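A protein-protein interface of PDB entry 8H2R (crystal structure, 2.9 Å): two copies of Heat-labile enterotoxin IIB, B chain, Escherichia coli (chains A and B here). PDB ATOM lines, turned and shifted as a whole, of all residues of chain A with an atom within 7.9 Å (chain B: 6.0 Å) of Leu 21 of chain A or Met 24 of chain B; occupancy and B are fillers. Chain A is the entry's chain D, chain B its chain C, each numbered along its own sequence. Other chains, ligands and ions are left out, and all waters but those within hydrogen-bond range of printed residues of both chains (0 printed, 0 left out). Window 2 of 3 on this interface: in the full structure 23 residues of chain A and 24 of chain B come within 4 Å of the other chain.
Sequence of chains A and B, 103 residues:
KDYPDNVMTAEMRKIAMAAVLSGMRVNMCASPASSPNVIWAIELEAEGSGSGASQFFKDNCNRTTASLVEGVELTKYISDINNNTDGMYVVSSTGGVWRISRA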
ATOM      1  N   LYS A  14     -37.775  31.401  -4.699  1.00  0.00           N
ATOM      2  CA  LYS A  14     -37.897  30.354  -3.691  1.00  0.00           C
ATOM      3  C   LYS A  14     -38.318  29.030  -4.314  1.00  0.00           C
ATOM      4  O   LYS A  14     -37.891  27.961  -3.862  1.00  0.00           O
ATOM      5  CB  LYS A  14     -38.917  30.756  -2.646  1.00  0.00           C
ATOM      6  CG  LYS A  14     -38.385  31.485  -1.500  1.00  0.00           C
ATOM      7  CD  LYS A  14     -39.399  31.396  -0.397  1.00  0.00           C
ATOM      8  CE  LYS A  14     -39.590  32.743   0.193  1.00  0.00           C
ATOM      9  NZ  LYS A  14     -39.841  33.631  -0.971  1.00  0.00           N
ATOM     10  N   ILE A  15     -39.180  29.079  -5.331  1.00  0.00           N
ATOM     11  CA  ILE A  15     -39.512  27.856  -6.050  1.00  0.00           C
ATOM     12  C   ILE A  15     -38.305  27.362  -6.833  1.00  0.00           C
ATOM     13  O   ILE A  15     -38.020  26.161  -6.877  1.00  0.00           O
ATOM     14  CB  ILE A  15     -40.717  28.077  -6.976  1.00  0.00           C
ATOM     15  CG1 ILE A  15     -41.945  28.507  -6.180  1.00  0.00           C
ATOM     16  CG2 ILE A  15     -41.004  26.798  -7.754  1.00  0.00           C
ATOM     17  CD1 ILE A  15     -43.254  28.053  -6.796  1.00  0.00           C
ATOM     18  N   ALA A  16     -37.590  28.274  -7.482  1.00  0.00           N
ATOM     19  CA  ALA A  16     -36.385  27.873  -8.185  1.00  0.00           C
ATOM     20  C   ALA A  16     -35.439  27.176  -7.234  1.00  0.00           C
ATOM     21  O   ALA A  16     -35.011  26.039  -7.479  1.00  0.00           O
ATOM     22  CB  ALA A  16     -35.709  29.084  -8.812  1.00  0.00           C
ATOM     23  N   MET A  17     -35.139  27.835  -6.115  1.00  0.00           N
ATOM     24  CA  MET A  17     -34.202  27.260  -5.171  1.00  0.00           C
ATOM     25  C   MET A  17     -34.715  25.928  -4.661  1.00  0.00           C
ATOM     26  O   MET A  17     -33.958  24.950  -4.592  1.00  0.00           O
ATOM     27  CB  MET A  17     -33.958  28.218  -4.023  1.00  0.00           C
ATOM     28  CG  MET A  17     -32.978  27.652  -3.049  1.00  0.00           C
ATOM     29  SD  MET A  17     -31.449  28.608  -3.162  1.00  0.00           S
ATOM     30  CE  MET A  17     -31.984  30.018  -2.228  1.00  0.00           C
ATOM     31  N   ALA A  18     -36.017  25.854  -4.356  1.00  0.00           N
ATOM     32  CA  ALA A  18     -36.601  24.583  -3.955  1.00  0.00           C
ATOM     33  C   ALA A  18     -36.385  23.533  -5.023  1.00  0.00           C
ATOM     34  O   ALA A  18     -36.189  22.365  -4.715  1.00  0.00           O
ATOM     35  CB  ALA A  18     -38.085  24.747  -3.668  1.00  0.00           C
ATOM     36  N   ALA A  19     -36.397  23.925  -6.288  1.00  0.00           N
ATOM     37  CA  ALA A  19     -36.283  22.907  -7.312  1.00  0.00           C
ATOM     38  C   ALA A  19     -34.883  22.343  -7.344  1.00  0.00           C
ATOM     39  O   ALA A  19     -34.702  21.127  -7.475  1.00  0.00           O
ATOM     40  CB  ALA A  19     -36.656  23.478  -8.668  1.00  0.00           C
ATOM     41  N   VAL A  20     -33.876  23.213  -7.210  1.00  0.00           N
ATOM     42  CA  VAL A  20     -32.492  22.767  -7.351  1.00  0.00           C
ATOM     43  C   VAL A  20     -32.043  22.023  -6.112  1.00  0.00           C
ATOM     44  O   VAL A  20     -31.431  20.954  -6.202  1.00  0.00           O
ATOM     45  CB  VAL A  20     -31.557  23.943  -7.650  1.00  0.00           C
ATOM     46  CG1 VAL A  20     -30.147  23.595  -7.221  1.00  0.00           C
ATOM     47  CG2 VAL A  20     -31.586  24.237  -9.122  1.00  0.00           C
ATOM     48  N   LEU A  21     -32.349  22.557  -4.933  1.00  0.00           N
ATOM     49  CA  LEU A  21     -31.968  21.821  -3.742  1.00  0.00           C
ATOM     50  C   LEU A  21     -32.680  20.494  -3.643  1.00  0.00           C
ATOM     51  O   LEU A  21     -32.431  19.758  -2.701  1.00  0.00           O
ATOM     52  CB  LEU A  21     -32.241  22.648  -2.492  1.00  0.00           C
ATOM     53  CG  LEU A  21     -31.461  23.942  -2.342  1.00  0.00           C
ATOM     54  CD1 LEU A  21     -32.030  24.683  -1.180  1.00  0.00           C
ATOM     55  CD2 LEU A  21     -29.999  23.654  -2.118  1.00  0.00           C
ATOM     56  N   SER A  22     -33.553  20.178  -4.585  1.00  0.00           N
ATOM     57  CA  SER A  22     -34.477  19.070  -4.450  1.00  0.00           C
ATOM     58  C   SER A  22     -34.575  18.207  -5.698  1.00  0.00           C
ATOM     59  O   SER A  22     -34.841  17.006  -5.612  1.00  0.00           O
ATOM     60  CB  SER A  22     -35.856  19.591  -4.155  1.00  0.00           C
ATOM     61  OG  SER A  22     -36.777  18.560  -4.257  1.00  0.00           O
ATOM     62  N   GLY A  23     -34.402  18.828  -6.868  1.00  0.00           N
ATOM     63  CA  GLY A  23     -34.613  18.093  -8.089  1.00  0.00           C
ATOM     64  C   GLY A  23     -36.031  17.624  -8.327  1.00  0.00           C
ATOM     65  O   GLY A  23     -36.241  16.785  -9.203  1.00  0.00           O
ATOM     66  N   MET A  24     -37.008  18.097  -7.555  1.00  0.00           N
ATOM     67  CA  MET A  24     -38.391  18.023  -8.000  1.00  0.00           C
ATOM     68  C   MET A  24     -38.491  18.840  -9.277  1.00  0.00           C
ATOM     69  O   MET A  24     -38.137  20.023  -9.270  1.00  0.00           O
ATOM     70  CB  MET A  24     -39.311  18.581  -6.909  1.00  0.00           C
ATOM     71  CG  MET A  24     -39.275  17.780  -5.587  1.00  0.00           C
ATOM     72  SD  MET A  24     -40.737  17.609  -4.535  1.00  0.00           S
ATOM     73  CE  MET A  24     -40.424  16.024  -3.757  1.00  0.00           C
ATOM     74  N   LEU A  74     -34.041  21.328 -12.701  1.00  0.00           N
ATOM     75  CA  LEU A  74     -33.164  22.451 -12.411  1.00  0.00           C
ATOM     76  C   LEU A  74     -31.969  21.914 -11.640  1.00  0.00           C
ATOM     77  O   LEU A  74     -32.141  21.258 -10.610  1.00  0.00           O
ATOM     78  CB  LEU A  74     -33.901  23.533 -11.632  1.00  0.00           C
ATOM     79  CG  LEU A  74     -35.025  24.183 -12.443  1.00  0.00           C
ATOM     80  CD1 LEU A  74     -35.532  25.436 -11.732  1.00  0.00           C
ATOM     81  CD2 LEU A  74     -34.595  24.493 -13.891  1.00  0.00           C
ATOM     82  N   THR A  75     -30.762  22.147 -12.158  1.00  0.00           N
ATOM     83  CA  THR A  75     -29.560  21.713 -11.466  1.00  0.00           C
ATOM     84  C   THR A  75     -28.641  22.852 -11.066  1.00  0.00           C
ATOM     85  O   THR A  75     -27.767  22.642 -10.214  1.00  0.00           O
ATOM     86  CB  THR A  75     -28.761  20.724 -12.326  1.00  0.00           C
ATOM     87  OG1 THR A  75     -28.725  21.224 -13.666  1.00  0.00           O
ATOM     88  CG2 THR A  75     -29.381  19.325 -12.292  1.00  0.00           C
ATOM     89  N   LYS A  76     -28.812  24.039 -11.629  1.00  0.00           N
ATOM     90  CA  LYS A  76     -27.980  25.159 -11.242  1.00  0.00           C
ATOM     91  C   LYS A  76     -28.825  26.392 -10.972  1.00  0.00           C
ATOM     92  O   LYS A  76     -29.696  26.746 -11.767  1.00  0.00           O
ATOM     93  CB  LYS A  76     -26.930  25.465 -12.314  1.00  0.00           C
ATOM     94  CG  LYS A  76     -25.846  24.418 -12.411  1.00  0.00           C
ATOM     95  CD  LYS A  76     -25.834  23.772 -13.781  1.00  0.00           C
ATOM     96  CE  LYS A  76     -24.565  22.958 -13.965  1.00  0.00           C
ATOM     97  NZ  LYS A  76     -24.053  22.429 -12.666  1.00  0.00           N
ATOM     98  N   TYR A  77     -28.533  27.052  -9.854  1.00  0.00           N
ATOM     99  CA  TYR A  77     -29.140  28.316  -9.465  1.00  0.00           C
ATOM    100  C   TYR A  77     -28.053  29.382  -9.490  1.00  0.00           C
ATOM    101  O   TYR A  77     -27.000  29.195  -8.871  1.00  0.00           O
ATOM    102  CB  TYR A  77     -29.767  28.194  -8.065  1.00  0.00           C
ATOM    103  CG  TYR A  77     -30.708  29.315  -7.670  1.00  0.00           C
ATOM    104  CD1 TYR A  77     -30.843  30.453  -8.456  1.00  0.00           C
ATOM    105  CD2 TYR A  77     -31.476  29.230  -6.516  1.00  0.00           C
ATOM    106  CE1 TYR A  77     -31.702  31.477  -8.096  1.00  0.00           C
ATOM    107  CE2 TYR A  77     -32.336  30.251  -6.148  1.00  0.00           C
ATOM    108  CZ  TYR A  77     -32.442  31.373  -6.943  1.00  0.00           C
ATOM    109  OH  TYR A  77     -33.293  32.403  -6.601  1.00  0.00           O
ATOM    110  N   ALA B  18     -26.938  27.737   1.483  1.00  0.00           N
ATOM    111  CA  ALA B  18     -27.411  26.421   1.082  1.00  0.00           C
ATOM    112  C   ALA B  18     -26.264  25.470   0.805  1.00  0.00           C
ATOM    113  O   ALA B  18     -26.312  24.300   1.189  1.00  0.00           O
ATOM    114  CB  ALA B  18     -28.297  26.546  -0.149  1.00  0.00           C
ATOM    115  N   ALA B  19     -25.228  25.946   0.121  1.00  0.00           N
ATOM    116  CA  ALA B  19     -24.116  25.076  -0.198  1.00  0.00           C
ATOM    117  C   ALA B  19     -23.358  24.651   1.043  1.00  0.00           C
ATOM    118  O   ALA B  19     -22.638  23.652   1.000  1.00  0.00           O
ATOM    119  CB  ALA B  19     -23.185  25.777  -1.165  1.00  0.00           C
ATOM    120  N   VAL B  20     -23.521  25.374   2.149  1.00  0.00           N
ATOM    121  CA  VAL B  20     -22.771  25.084   3.366  1.00  0.00           C
ATOM    122  C   VAL B  20     -23.455  24.019   4.200  1.00  0.00           C
ATOM    123  O   VAL B  20     -22.775  23.227   4.863  1.00  0.00           O
ATOM    124  CB  VAL B  20     -22.544  26.363   4.203  1.00  0.00           C
ATOM    125  CG1 VAL B  20     -21.998  26.020   5.554  1.00  0.00           C
ATOM    126  CG2 VAL B  20     -21.550  27.300   3.520  1.00  0.00           C
ATOM    127  N   LEU B  21     -24.789  23.991   4.192  1.00  0.00           N
ATOM    128  CA  LEU B  21     -25.555  22.993   4.938  1.00  0.00           C
ATOM    129  C   LEU B  21     -25.752  21.703   4.165  1.00  0.00           C
ATOM    130  O   LEU B  21     -26.053  20.681   4.781  1.00  0.00           O
ATOM    131  CB  LEU B  21     -26.930  23.547   5.327  1.00  0.00           C
ATOM    132  CG  LEU B  21     -26.922  24.991   5.846  1.00  0.00           C
ATOM    133  CD1 LEU B  21     -28.216  25.728   5.515  1.00  0.00           C
ATOM    134  CD2 LEU B  21     -26.654  25.026   7.334  1.00  0.00           C
ATOM    135  N   SER B  22     -25.555  21.720   2.848  1.00  0.00           N
ATOM    136  CA  SER B  22     -25.850  20.595   1.978  1.00  0.00           C
ATOM    137  C   SER B  22     -24.643  20.013   1.281  1.00  0.00           C
ATOM    138  O   SER B  22     -24.813  19.118   0.448  1.00  0.00           O
ATOM    139  CB  SER B  22     -26.836  21.008   0.887  1.00  0.00           C
ATOM    140  OG  SER B  22     -26.159  21.805  -0.060  1.00  0.00           O
ATOM    141  N   GLY B  23     -23.446  20.531   1.529  1.00  0.00           N
ATOM    142  CA  GLY B  23     -22.289  20.052   0.820  1.00  0.00           C
ATOM    143  C   GLY B  23     -22.264  20.349  -0.659  1.00  0.00           C
ATOM    144  O   GLY B  23     -21.276  20.007  -1.318  1.00  0.00           O
ATOM    145  N   MET B  24     -23.302  20.965  -1.217  1.00  0.00           N
ATOM    146  CA  MET B  24     -23.234  21.301  -2.629  1.00  0.00           C
ATOM    147  C   MET B  24     -22.114  22.272  -2.903  1.00  0.00           C
ATOM    148  O   MET B  24     -21.695  23.045  -2.032  1.00  0.00           O
ATOM    149  CB  MET B  24     -24.505  21.930  -3.146  1.00  0.00           C
ATOM    150  CG  MET B  24     -25.484  20.898  -3.522  1.00  0.00           C
ATOM    151  SD  MET B  24     -26.997  21.700  -3.993  1.00  0.00           S
ATOM    152  CE  MET B  24     -28.134  20.442  -3.470  1.00  0.00           C
ATOM    153  N   ARG B  25     -21.648  22.231  -4.138  1.00  0.00           N
ATOM    154  CA  ARG B  25     -20.541  23.044  -4.588  1.00  0.00           C
ATOM    155  C   ARG B  25     -21.089  24.244  -5.331  1.00  0.00           C
ATOM    156  O   ARG B  25     -22.205  24.213  -5.842  1.00  0.00           O
ATOM    157  CB  ARG B  25     -19.627  22.227  -5.490  1.00  0.00           C
ATOM    158  CG  ARG B  25     -19.838  20.724  -5.317  1.00  0.00           C
ATOM    159  CD  ARG B  25     -18.983  20.128  -4.193  1.00  0.00           C
ATOM    160  NE  ARG B  25     -17.610  19.899  -4.635  1.00  0.00           N
ATOM    161  CZ  ARG B  25     -16.707  19.186  -3.971  1.00  0.00           C
ATOM    162  NH1 ARG B  25     -17.003  18.594  -2.821  1.00  0.00           N
ATOM    163  NH2 ARG B  25     -15.480  19.057  -4.478  1.00  0.00           N
ATOM    164  N   VAL B  26     -20.313  25.321  -5.350  1.00  0.00           N
ATOM    165  CA  VAL B  26     -20.662  26.479  -6.151  1.00  0.00           C
ATOM    166  C   VAL B  26     -19.474  26.821  -7.033  1.00  0.00           C
ATOM    167  O   VAL B  26     -18.329  26.478  -6.743  1.00  0.00           O
ATOM    168  CB  VAL B  26     -21.084  27.710  -5.314  1.00  0.00           C
ATOM    169  CG1 VAL B  26     -22.063  27.321  -4.252  1.00  0.00           C
ATOM    170  CG2 VAL B  26     -19.888  28.401  -4.726  1.00  0.00           C
ATOM    171  N   LEU B  44     -25.147  27.894  -7.746  1.00  0.00           N
ATOM    172  CA  LEU B  44     -25.262  26.697  -6.923  1.00  0.00           C
ATOM    173  C   LEU B  44     -25.548  25.507  -7.822  1.00  0.00           C
ATOM    174  O   LEU B  44     -26.390  25.596  -8.719  1.00  0.00           O
ATOM    175  CB  LEU B  44     -26.357  26.855  -5.870  1.00  0.00           C
ATOM    176  CG  LEU B  44     -26.635  25.620  -5.025  1.00  0.00           C
ATOM    177  CD1 LEU B  44     -25.647  25.518  -3.863  1.00  0.00           C
ATOM    178  CD2 LEU B  44     -28.048  25.700  -4.489  1.00  0.00           C
ATOM    179  N   GLU B  45     -24.833  24.406  -7.610  1.00  0.00           N
ATOM    180  CA  GLU B  45     -24.917  23.288  -8.530  1.00  0.00           C
ATOM    181  C   GLU B  45     -25.183  22.002  -7.772  1.00  0.00           C
ATOM    182  O   GLU B  45     -24.398  21.608  -6.908  1.00  0.00           O
ATOM    183  CB  GLU B  45     -23.652  23.186  -9.380  1.00  0.00           C
ATOM    184  CG  GLU B  45     -22.349  22.812  -8.690  1.00  0.00           C
ATOM    185  CD  GLU B  45     -21.171  22.854  -9.660  1.00  0.00           C
ATOM    186  OE1 GLU B  45     -21.269  23.579 -10.677  1.00  0.00           O
ATOM    187  OE2 GLU B  45     -20.161  22.150  -9.428  1.00  0.00           O
ATOM    188  N   ALA B  46     -26.300  21.351  -8.084  1.00  0.00           N
ATOM    189  CA  ALA B  46     -26.551  20.049  -7.487  1.00  0.00           C
ATOM    190  C   ALA B  46     -25.561  19.011  -7.993  1.00  0.00           C
ATOM    191  O   ALA B  46     -25.116  18.156  -7.225  1.00  0.00           O
ATOM    192  CB  ALA B  46     -27.975  19.598  -7.779  1.00  0.00           C
ATOM    193  N   VAL B  72     -16.018  25.007  -6.098  1.00  0.00           N
ATOM    194  CA  VAL B  72     -15.608  25.326  -4.731  1.00  0.00           C
ATOM    195  C   VAL B  72     -16.592  24.701  -3.744  1.00  0.00           C
ATOM    196  O   VAL B  72     -17.805  24.934  -3.841  1.00  0.00           O
ATOM    197  CB  VAL B  72     -15.559  26.851  -4.540  1.00  0.00           C
ATOM    198  CG1 VAL B  72     -15.466  27.211  -3.062  1.00  0.00           C
ATOM    199  CG2 VAL B  72     -14.438  27.455  -5.322  1.00  0.00           C
ATOM    200  N   GLU B  73     -16.079  23.923  -2.773  1.00  0.00           N
ATOM    201  CA  GLU B  73     -16.902  23.387  -1.682  1.00  0.00           C
ATOM    202  C   GLU B  73     -16.765  24.290  -0.472  1.00  0.00           C
ATOM    203  O   GLU B  73     -15.714  24.306   0.167  1.00  0.00           O
ATOM    204  CB  GLU B  73     -16.525  21.955  -1.298  1.00  0.00           C
ATOM    205  CG  GLU B  73     -17.769  21.097  -0.938  1.00  0.00           C
ATOM    206  CD  GLU B  73     -17.478  19.924   0.007  1.00  0.00           C
ATOM    207  OE1 GLU B  73     -16.282  19.585   0.186  1.00  0.00           O
ATOM    208  OE2 GLU B  73     -18.450  19.338   0.566  1.00  0.00           O
ATOM    209  N   LEU B  74     -17.838  25.011  -0.142  1.00  0.00           N
ATOM    210  CA  LEU B  74     -17.797  25.981   0.949  1.00  0.00           C
ATOM    211  C   LEU B  74     -17.885  25.294   2.309  1.00  0.00           C
ATOM    212  O   LEU B  74     -18.545  24.264   2.461  1.00  0.00           O
ATOM    213  CB  LEU B  74     -18.920  27.002   0.794  1.00  0.00           C
ATOM    214  CG  LEU B  74     -18.802  27.859  -0.469  1.00  0.00           C
ATOM    215  CD1 LEU B  74     -20.145  28.467  -0.867  1.00  0.00           C
ATOM    216  CD2 LEU B  74     -17.750  28.951  -0.286  1.00  0.00           C
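The backbone NH (N) of Ala 46 of chain B lies within hydrogen-bond range of the backbone carbonyl oxygen (O) of Thr 75 of chain A, 2.9 Å away.
The side-chain carboxylate (OE1) of Glu 45 of chain B lies within salt-bridge range of the side-chain amino group (NZ) of Lys 76 of chain A (3.6 Å).
The backbone NH of Leu 44 of chain B lies within hydrogen-bond range of the backbone carbonyl oxygen of Tyr 77 of chain A (2.5 Å).
Of chain B, only Ala 18 (3.9 Å), Met 24 (3.95 Å) and Leu 44 (3.7 Å) come within 4 Å of Leu 21 of chain A.
Of chain A, only Leu 21 (3.95 Å) comes within 4 Å of Met 24 of chain B.
Printed residues of chain A within 4 Å of Leu 44 of chain B: Leu 21, Thr 75, Lys 76 and Tyr 77.
Of the printed residues of chain A, Glu 45 of chain B touches Thr 75 and Lys 76.
Printed residues of chain A within 4 Å of Ala 46 of chain B: Thr 75.
Met 24 of chain A touches none of the printed residues of chain B.
The nearest printed residue of chain A that does not touch Ala 18 of chain B is Met 17 of chain A (4.8 Å).
Leu 21 of chain A touches Ala 18 of chain B, but with the chains exchanged Ala 18 of chain A does not touch Leu 21 of chain B (12.6 Å).
Leu 21 of chain A touches Met 24 of chain B, but with the chains exchanged Met 24 of chain A does not touch Leu 21 of chain B (16.6 Å).
Leu 21 of chain A touches Ala 18 of chain B (CD2 to CB, 3.9 Å).
Met 24 of chain B touches Leu 21 of chain A.
Leu 21 of chain A touches Leu 44 of chain B (CD2 to CD2, 3.7 Å).
O of Leu 44 of chain B touches O of Thr 75 of chain A (3.6 Å).
O of Thr 75 of chain A touches CA of Glu 45 of chain B, 3.4 Å away.
Lys 76 of chain A touches Leu 44 of chain B (CA to O, 3.0 Å).
The backbone carbonyl oxygen of Arg 25 of chain B lies within hydrogen-bond range of the backbone NH of Glu 45 of chain B (3.2 Å).
The side-chain hydroxyl of Ser 22 of chain B is in hydrogen-bond range of the backbone carbonyl oxygen of Ala 18 of chain B (2.8 Å).
N of Met 24 of chain B sits close to OG of Ser 22 of chain B, at 3.2 Å.
Hydrophobic or aromatic side chains of chain A within 4 Å of the printed part of chain B: Leu 21.
Among the printed residues, 9 pairs touch across the chains.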
